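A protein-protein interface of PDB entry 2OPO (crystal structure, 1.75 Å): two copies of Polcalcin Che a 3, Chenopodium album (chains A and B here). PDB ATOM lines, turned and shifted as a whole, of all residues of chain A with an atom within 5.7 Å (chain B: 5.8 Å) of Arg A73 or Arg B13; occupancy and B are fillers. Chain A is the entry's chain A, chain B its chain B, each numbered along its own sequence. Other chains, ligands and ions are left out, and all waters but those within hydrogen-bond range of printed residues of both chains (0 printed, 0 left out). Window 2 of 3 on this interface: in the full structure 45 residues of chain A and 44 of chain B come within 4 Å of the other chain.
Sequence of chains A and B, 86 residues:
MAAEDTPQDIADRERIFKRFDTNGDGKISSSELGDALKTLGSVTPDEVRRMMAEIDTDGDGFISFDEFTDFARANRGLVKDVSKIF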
ATOM      1  N   PHE A  65      -0.928 -32.202  -6.622  1.00  0.00           N
ATOM      2  CA  PHE A  65      -0.401 -30.914  -6.130  1.00  0.00           C
ATOM      3  C   PHE A  65       1.146 -30.871  -6.240  1.00  0.00           C
ATOM      4  O   PHE A  65       1.706 -29.835  -6.545  1.00  0.00           O
ATOM      5  CB  PHE A  65      -0.814 -30.624  -4.700  1.00  0.00           C
ATOM      6  CG  PHE A  65      -0.417 -29.276  -4.232  1.00  0.00           C
ATOM      7  CD1 PHE A  65      -1.045 -28.120  -4.706  1.00  0.00           C
ATOM      8  CD2 PHE A  65       0.651 -29.133  -3.370  1.00  0.00           C
ATOM      9  CE1 PHE A  65      -0.654 -26.887  -4.276  1.00  0.00           C
ATOM     10  CE2 PHE A  65       1.074 -27.882  -3.020  1.00  0.00           C
ATOM     11  CZ  PHE A  65       0.404 -26.764  -3.457  1.00  0.00           C
ATOM     12  N   PHE A  68       2.012 -30.161  -9.818  1.00  0.00           N
ATOM     13  CA  PHE A  68       1.665 -28.743 -10.092  1.00  0.00           C
ATOM     14  C   PHE A  68       2.748 -27.865  -9.498  1.00  0.00           C
ATOM     15  O   PHE A  68       3.242 -26.909 -10.167  1.00  0.00           O
ATOM     16  CB  PHE A  68       0.276 -28.460  -9.472  1.00  0.00           C
ATOM     17  CG  PHE A  68      -0.189 -27.016  -9.624  1.00  0.00           C
ATOM     18  CD1 PHE A  68      -0.840 -26.620 -10.779  1.00  0.00           C
ATOM     19  CD2 PHE A  68       0.003 -26.108  -8.627  1.00  0.00           C
ATOM     20  CE1 PHE A  68      -1.286 -25.329 -10.905  1.00  0.00           C
ATOM     21  CE2 PHE A  68      -0.423 -24.794  -8.755  1.00  0.00           C
ATOM     22  CZ  PHE A  68      -1.059 -24.418  -9.893  1.00  0.00           C
ATOM     23  N   THR A  69       3.169 -28.211  -8.269  1.00  0.00           N
ATOM     24  CA  THR A  69       4.253 -27.441  -7.596  1.00  0.00           C
ATOM     25  C   THR A  69       5.552 -27.511  -8.374  1.00  0.00           C
ATOM     26  O   THR A  69       6.217 -26.483  -8.570  1.00  0.00           O
ATOM     27  CB  THR A  69       4.526 -27.896  -6.191  1.00  0.00           C
ATOM     28  OG1 THR A  69       3.379 -27.647  -5.372  1.00  0.00           O
ATOM     29  CG2 THR A  69       5.755 -27.095  -5.595  1.00  0.00           C
ATOM     30  N   ASP A  70       5.937 -28.699  -8.800  1.00  0.00           N
ATOM     31  CA  ASP A  70       7.145 -28.862  -9.648  1.00  0.00           C
ATOM     32  C   ASP A  70       7.091 -27.968 -10.889  1.00  0.00           C
ATOM     33  O   ASP A  70       8.067 -27.302 -11.249  1.00  0.00           O
ATOM     34  CB  ASP A  70       7.292 -30.322 -10.096  1.00  0.00           C
ATOM     35  CG  ASP A  70       7.588 -31.266  -8.956  1.00  0.00           C
ATOM     36  OD1 ASP A  70       8.099 -30.865  -7.890  1.00  0.00           O
ATOM     37  OD2 ASP A  70       7.284 -32.464  -9.133  1.00  0.00           O
ATOM     38  N   PHE A  71       5.919 -27.898 -11.528  1.00  0.00           N
ATOM     39  CA  PHE A  71       5.732 -27.027 -12.690  1.00  0.00           C
ATOM     40  C   PHE A  71       5.877 -25.543 -12.280  1.00  0.00           C
ATOM     41  O   PHE A  71       6.589 -24.743 -12.921  1.00  0.00           O
ATOM     42  CB  PHE A  71       4.347 -27.336 -13.331  1.00  0.00           C
ATOM     43  CG  PHE A  71       4.073 -26.540 -14.541  1.00  0.00           C
ATOM     44  CD1 PHE A  71       4.663 -26.877 -15.751  1.00  0.00           C
ATOM     45  CD2 PHE A  71       3.294 -25.407 -14.463  1.00  0.00           C
ATOM     46  CE1 PHE A  71       4.411 -26.100 -16.905  1.00  0.00           C
ATOM     47  CE2 PHE A  71       3.081 -24.589 -15.588  1.00  0.00           C
ATOM     48  CZ  PHE A  71       3.660 -24.959 -16.807  1.00  0.00           C
ATOM     49  N   ALA A  72       5.254 -25.189 -11.174  1.00  0.00           N
ATOM     50  CA  ALA A  72       5.233 -23.819 -10.685  1.00  0.00           C
ATOM     51  C   ALA A  72       6.628 -23.354 -10.266  1.00  0.00           C
ATOM     52  O   ALA A  72       7.002 -22.229 -10.562  1.00  0.00           O
ATOM     53  CB  ALA A  72       4.273 -23.721  -9.496  1.00  0.00           C
ATOM     54  N   ARG A  73       7.392 -24.222  -9.607  1.00  0.00           N
ATOM     55  CA  ARG A  73       8.760 -23.878  -9.184  1.00  0.00           C
ATOM     56  C   ARG A  73       9.662 -23.555 -10.396  1.00  0.00           C
ATOM     57  O   ARG A  73      10.605 -22.705 -10.301  1.00  0.00           O
ATOM     58  CB  ARG A  73       9.367 -25.000  -8.308  1.00  0.00           C
ATOM     59  CG  ARG A  73       8.764 -25.111  -6.896  1.00  0.00           C
ATOM     60  CD  ARG A  73       9.665 -25.929  -5.953  1.00  0.00           C
ATOM     61  NE  ARG A  73       9.009 -26.357  -4.713  1.00  0.00           N
ATOM     62  CZ  ARG A  73       8.718 -25.560  -3.683  1.00  0.00           C
ATOM     63  NH1 ARG A  73       9.003 -24.256  -3.723  1.00  0.00           N
ATOM     64  NH2 ARG A  73       8.131 -26.070  -2.604  1.00  0.00           N
ATOM     65  N   ALA A  74       9.390 -24.210 -11.520  1.00  0.00           N
ATOM     66  CA  ALA A  74      10.112 -24.020 -12.770  1.00  0.00           C
ATOM     67  C   ALA A  74       9.620 -22.834 -13.585  1.00  0.00           C
ATOM     68  O   ALA A  74      10.304 -22.375 -14.502  1.00  0.00           O
ATOM     69  CB  ALA A  74       9.982 -25.286 -13.606  1.00  0.00           C
ATOM     70  N   ASN A  75       8.421 -22.362 -13.284  1.00  0.00           N
ATOM     71  CA  ASN A  75       7.801 -21.272 -13.999  1.00  0.00           C
ATOM     72  C   ASN A  75       7.222 -20.264 -13.012  1.00  0.00           C
ATOM     73  O   ASN A  75       6.031 -20.044 -13.009  1.00  0.00           O
ATOM     74  CB  ASN A  75       6.687 -21.813 -14.927  1.00  0.00           C
ATOM     75  CG  ASN A  75       7.202 -22.827 -15.934  1.00  0.00           C
ATOM     76  OD1 ASN A  75       7.614 -22.471 -17.057  1.00  0.00           O
ATOM     77  ND2 ASN A  75       7.235 -24.098 -15.524  1.00  0.00           N
ATOM     78  N   ARG A  76       8.064 -19.603 -12.228  1.00  0.00           N
ATOM     79  CA  ARG A  76       7.584 -18.645 -11.209  1.00  0.00           C
ATOM     80  C   ARG A  76       6.684 -17.532 -11.769  1.00  0.00           C
ATOM     81  O   ARG A  76       5.731 -17.103 -11.105  1.00  0.00           O
ATOM     82  CB  ARG A  76       8.742 -18.024 -10.409  1.00  0.00           C
ATOM     83  CG  ARG A  76       8.985 -18.630  -9.008  1.00  0.00           C
ATOM     84  CD  ARG A  76      10.122 -19.681  -8.945  1.00  0.00           C
ATOM     85  NE  ARG A  76      10.165 -20.347  -7.636  1.00  0.00           N
ATOM     86  CZ  ARG A  76      10.969 -21.362  -7.282  1.00  0.00           C
ATOM     87  NH1 ARG A  76      11.859 -21.873  -8.128  1.00  0.00           N
ATOM     88  NH2 ARG A  76      10.892 -21.874  -6.054  1.00  0.00           N
ATOM     89  N   VAL A  79       2.484 -18.588 -11.465  1.00  0.00           N
ATOM     90  CA  VAL A  79       1.591 -18.344 -10.357  1.00  0.00           C
ATOM     91  C   VAL A  79       1.439 -16.876 -10.099  1.00  0.00           C
ATOM     92  O   VAL A  79       0.342 -16.402  -9.842  1.00  0.00           O
ATOM     93  CB  VAL A  79       2.125 -19.045  -9.057  1.00  0.00           C
ATOM     94  CG1 VAL A  79       1.466 -18.487  -7.769  1.00  0.00           C
ATOM     95  CG2 VAL A  79       1.941 -20.525  -9.166  1.00  0.00           C
ATOM     96  N   GLN B   8       2.626 -17.272   2.089  1.00  0.00           N
ATOM     97  CA  GLN B   8       1.862 -16.673   0.979  1.00  0.00           C
ATOM     98  C   GLN B   8       2.153 -17.337  -0.369  1.00  0.00           C
ATOM     99  O   GLN B   8       1.243 -17.460  -1.203  1.00  0.00           O
ATOM    100  CB  GLN B   8       2.065 -15.146   0.891  1.00  0.00           C
ATOM    101  CG  GLN B   8       0.956 -14.408   0.087  1.00  0.00           C
ATOM    102  CD  GLN B   8      -0.458 -14.540   0.686  1.00  0.00           C
ATOM    103  OE1 GLN B   8      -0.693 -14.205   1.859  1.00  0.00           O
ATOM    104  NE2 GLN B   8      -1.405 -15.022  -0.124  1.00  0.00           N
ATOM    105  N   ASP B   9       3.400 -17.767  -0.581  1.00  0.00           N
ATOM    106  CA  ASP B   9       3.805 -18.436  -1.844  1.00  0.00           C
ATOM    107  C   ASP B   9       3.010 -19.738  -2.086  1.00  0.00           C
ATOM    108  O   ASP B   9       2.520 -20.004  -3.181  1.00  0.00           O
ATOM    109  CB  ASP B   9       5.309 -18.769  -1.805  1.00  0.00           C
ATOM    110  CG  ASP B   9       6.190 -17.533  -1.767  1.00  0.00           C
ATOM    111  OD1 ASP B   9       5.664 -16.417  -2.007  1.00  0.00           O
ATOM    112  OD2 ASP B   9       7.408 -17.678  -1.489  1.00  0.00           O
ATOM    113  N   ILE B  10       2.906 -20.541  -1.032  1.00  0.00           N
ATOM    114  CA  ILE B  10       2.081 -21.755  -1.067  1.00  0.00           C
ATOM    115  C   ILE B  10       0.608 -21.388  -1.178  1.00  0.00           C
ATOM    116  O   ILE B  10      -0.123 -21.995  -1.979  1.00  0.00           O
ATOM    117  CB  ILE B  10       2.281 -22.612   0.194  1.00  0.00           C
ATOM    118  CG1 ILE B  10       3.775 -22.808   0.453  1.00  0.00           C
ATOM    119  CG2 ILE B  10       1.524 -23.964   0.086  1.00  0.00           C
ATOM    120  CD1 ILE B  10       4.614 -22.917  -0.804  1.00  0.00           C
ATOM    121  N   ALA B  11       0.165 -20.413  -0.377  1.00  0.00           N
ATOM    122  CA  ALA B  11      -1.259 -20.019  -0.357  1.00  0.00           C
ATOM    123  C   ALA B  11      -1.733 -19.670  -1.774  1.00  0.00           C
ATOM    124  O   ALA B  11      -2.871 -19.986  -2.199  1.00  0.00           O
ATOM    125  CB  ALA B  11      -1.494 -18.857   0.598  1.00  0.00           C
ATOM    126  N   ASP B  12      -0.836 -19.021  -2.512  1.00  0.00           N
ATOM    127  CA  ASP B  12      -1.095 -18.692  -3.892  1.00  0.00           C
ATOM    128  C   ASP B  12      -1.186 -19.877  -4.831  1.00  0.00           C
ATOM    129  O   ASP B  12      -2.006 -19.912  -5.764  1.00  0.00           O
ATOM    130  CB  ASP B  12       0.045 -17.862  -4.424  1.00  0.00           C
ATOM    131  CG  ASP B  12      -0.209 -16.395  -4.326  1.00  0.00           C
ATOM    132  OD1 ASP B  12      -0.646 -15.918  -3.229  1.00  0.00           O
ATOM    133  OD2 ASP B  12       0.071 -15.745  -5.368  1.00  0.00           O
ATOM    134  N   ARG B  13      -0.233 -20.788  -4.680  1.00  0.00           N
ATOM    135  CA  ARG B  13      -0.178 -21.976  -5.520  1.00  0.00           C
ATOM    136  C   ARG B  13      -1.412 -22.829  -5.257  1.00  0.00           C
ATOM    137  O   ARG B  13      -2.053 -23.383  -6.184  1.00  0.00           O
ATOM    138  CB  ARG B  13       1.081 -22.776  -5.171  1.00  0.00           C
ATOM    139  CG  ARG B  13       1.731 -23.464  -6.335  1.00  0.00           C
ATOM    140  CD  ARG B  13       3.166 -23.796  -5.960  1.00  0.00           C
ATOM    141  NE  ARG B  13       3.153 -24.776  -4.894  1.00  0.00           N
ATOM    142  CZ  ARG B  13       3.991 -24.826  -3.872  1.00  0.00           C
ATOM    143  NH1 ARG B  13       4.980 -23.948  -3.734  1.00  0.00           N
ATOM    144  NH2 ARG B  13       3.828 -25.778  -2.992  1.00  0.00           N
ATOM    145  N   GLU B  14      -1.743 -22.952  -3.998  1.00  0.00           N
ATOM    146  CA  GLU B  14      -2.888 -23.758  -3.628  1.00  0.00           C
ATOM    147  C   GLU B  14      -4.171 -23.120  -4.158  1.00  0.00           C
ATOM    148  O   GLU B  14      -5.059 -23.830  -4.579  1.00  0.00           O
ATOM    149  CB  GLU B  14      -2.911 -24.063  -2.129  1.00  0.00           C
ATOM    150  CG  GLU B  14      -3.503 -23.080  -1.220  1.00  0.00           C
ATOM    151  CD  GLU B  14      -3.352 -23.489   0.240  1.00  0.00           C
ATOM    152  OE1 GLU B  14      -4.043 -24.458   0.668  1.00  0.00           O
ATOM    153  OE2 GLU B  14      -2.566 -22.842   0.946  1.00  0.00           O
ATOM    154  N   ARG B  15      -4.232 -21.782  -4.174  1.00  0.00           N
ATOM    155  CA  ARG B  15      -5.443 -21.127  -4.677  1.00  0.00           C
ATOM    156  C   ARG B  15      -5.681 -21.436  -6.172  1.00  0.00           C
ATOM    157  O   ARG B  15      -6.814 -21.778  -6.519  1.00  0.00           O
ATOM    158  CB  ARG B  15      -5.454 -19.627  -4.334  1.00  0.00           C
ATOM    159  CG  ARG B  15      -6.829 -18.951  -4.518  1.00  0.00           C
ATOM    160  CD  ARG B  15      -6.765 -17.420  -4.351  1.00  0.00           C
ATOM    161  NE  ARG B  15      -5.474 -16.884  -4.798  1.00  0.00           N
ATOM    162  CZ  ARG B  15      -5.144 -16.662  -6.063  1.00  0.00           C
ATOM    163  NH1 ARG B  15      -6.011 -16.883  -7.049  1.00  0.00           N
ATOM    164  NH2 ARG B  15      -3.933 -16.206  -6.345  1.00  0.00           N
ATOM    165  N   ILE B  16      -4.663 -21.435  -7.023  1.00  0.00           N
ATOM    166  CA  ILE B  16      -4.815 -21.793  -8.425  1.00  0.00           C
ATOM    167  C   ILE B  16      -5.194 -23.279  -8.538  1.00  0.00           C
ATOM    168  O   ILE B  16      -6.051 -23.656  -9.341  1.00  0.00           O
ATOM    169  CB  ILE B  16      -3.530 -21.565  -9.236  1.00  0.00           C
ATOM    170  CG1 ILE B  16      -2.982 -20.129  -9.124  1.00  0.00           C
ATOM    171  CG2 ILE B  16      -3.706 -21.883 -10.694  1.00  0.00           C
ATOM    172  CD1 ILE B  16      -1.710 -19.972  -9.932  1.00  0.00           C
ATOM    173  N   PHE B  17      -4.473 -24.129  -7.783  1.00  0.00           N
ATOM    174  CA  PHE B  17      -4.724 -25.588  -7.865  1.00  0.00           C
ATOM    175  C   PHE B  17      -6.169 -25.857  -7.520  1.00  0.00           C
ATOM    176  O   PHE B  17      -6.856 -26.559  -8.245  1.00  0.00           O
ATOM    177  CB  PHE B  17      -3.787 -26.380  -6.911  1.00  0.00           C
ATOM    178  CG  PHE B  17      -3.924 -27.852  -7.026  1.00  0.00           C
ATOM    179  CD1 PHE B  17      -3.193 -28.575  -7.945  1.00  0.00           C
ATOM    180  CD2 PHE B  17      -4.870 -28.532  -6.245  1.00  0.00           C
ATOM    181  CE1 PHE B  17      -3.310 -29.942  -8.006  1.00  0.00           C
ATOM    182  CE2 PHE B  17      -5.009 -29.893  -6.350  1.00  0.00           C
ATOM    183  CZ  PHE B  17      -4.296 -30.565  -7.239  1.00  0.00           C
ATOM    184  N   LYS B  18      -6.639 -25.286  -6.419  1.00  0.00           N
ATOM    185  CA  LYS B  18      -8.029 -25.537  -5.991  1.00  0.00           C
ATOM    186  C   LYS B  18      -9.019 -24.947  -6.994  1.00  0.00           C
ATOM    187  O   LYS B  18     -10.087 -25.515  -7.147  1.00  0.00           O
ATOM    188  CB  LYS B  18      -8.252 -24.966  -4.589  1.00  0.00           C
ATOM    189  CG  LYS B  18      -7.431 -25.741  -3.536  1.00  0.00           C
ATOM    190  CD  LYS B  18      -7.577 -25.227  -2.125  1.00  0.00           C
ATOM    191  CE  LYS B  18      -6.562 -25.849  -1.140  1.00  0.00           C
ATOM    192  NZ  LYS B  18      -6.783 -25.332   0.282  1.00  0.00           N
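NE of Arg B13 is in hydrogen-bond range of OG1 of Thr A69, at 2.9 Å.
The backbone carbonyl oxygen of Phe A65 lies within hydrogen-bond range of the side-chain hydroxyl of Thr A69 (3.0 Å).
The guanidinium group (NH1) of Arg A76 is in hydrogen-bond range of the backbone carbonyl oxygen (O) of Arg A73, 2.6 Å away.
NE2 of Gln B8 sits at hydrogen-bond distance from OD1 of Asp B12 (3.3 Å).
OE1 of Glu B14 lies within salt-bridge range of NZ of Lys B18 (2.9 Å).
Among the printed residues, merely in contact across the chains: Phe A65 with Arg B13 (3.5 Å), Phe A65 with Glu B14 (3.9 Å), Phe A65 with Phe B17 (3.6 Å), Phe A68 with Arg B13 (3.4 Å), Phe A68 with Ile B16 (3.8 Å), Phe A68 with Phe B17 (3.8 Å), Ala A72 with Arg B13 (3.7 Å), Arg A73 with Arg B13 (3.96 Å), Val A79 with Asp B12 (3.7 Å) and Val A79 with Ile B16 (3.7 Å).
Printed residues of chain B within 4 Å of Thr A69: Arg B13 (2.9 Å).
Printed residues of chain B within 4 Å of Ala A72: Arg B13.
Of the printed residues of chain B, Arg A73 touches Arg B13.
Ala B11 touches none of the printed residues of chain A.
Printed residues of chain A within 4 Å of Asp B12: Val A79.
Of the printed residues of chain A, Arg B13 touches Phe A65, Phe A68, Thr A69, Ala A72 and Arg A73.
Printed residues of chain A within 4 Å of Phe B17: Phe A65 (3.6 Å) and Phe A68 (3.8 Å).
The nearest printed residue of chain B that does not touch Arg A73 is Ile B10 (5.1 Å).
The nearest printed residue of chain A that does not touch Arg B13 is Val A79 (4.1 Å).
The nearest printed residue of chain A that does not touch Ile B16 is Ala A72 (7.1 Å).
Of the 11 printed residues of chain A, 6 touch a printed residue of chain B.
Hydrophobic or aromatic side chains of chain A that line the printed part of chain B: Phe A65, Phe A68, Ala A72 and Val A79.
Hydrophobic or aromatic side chains of chain B within 4 Å of the printed part of chain A: Ile B16 and Phe B17.
No position is printed for both chains.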
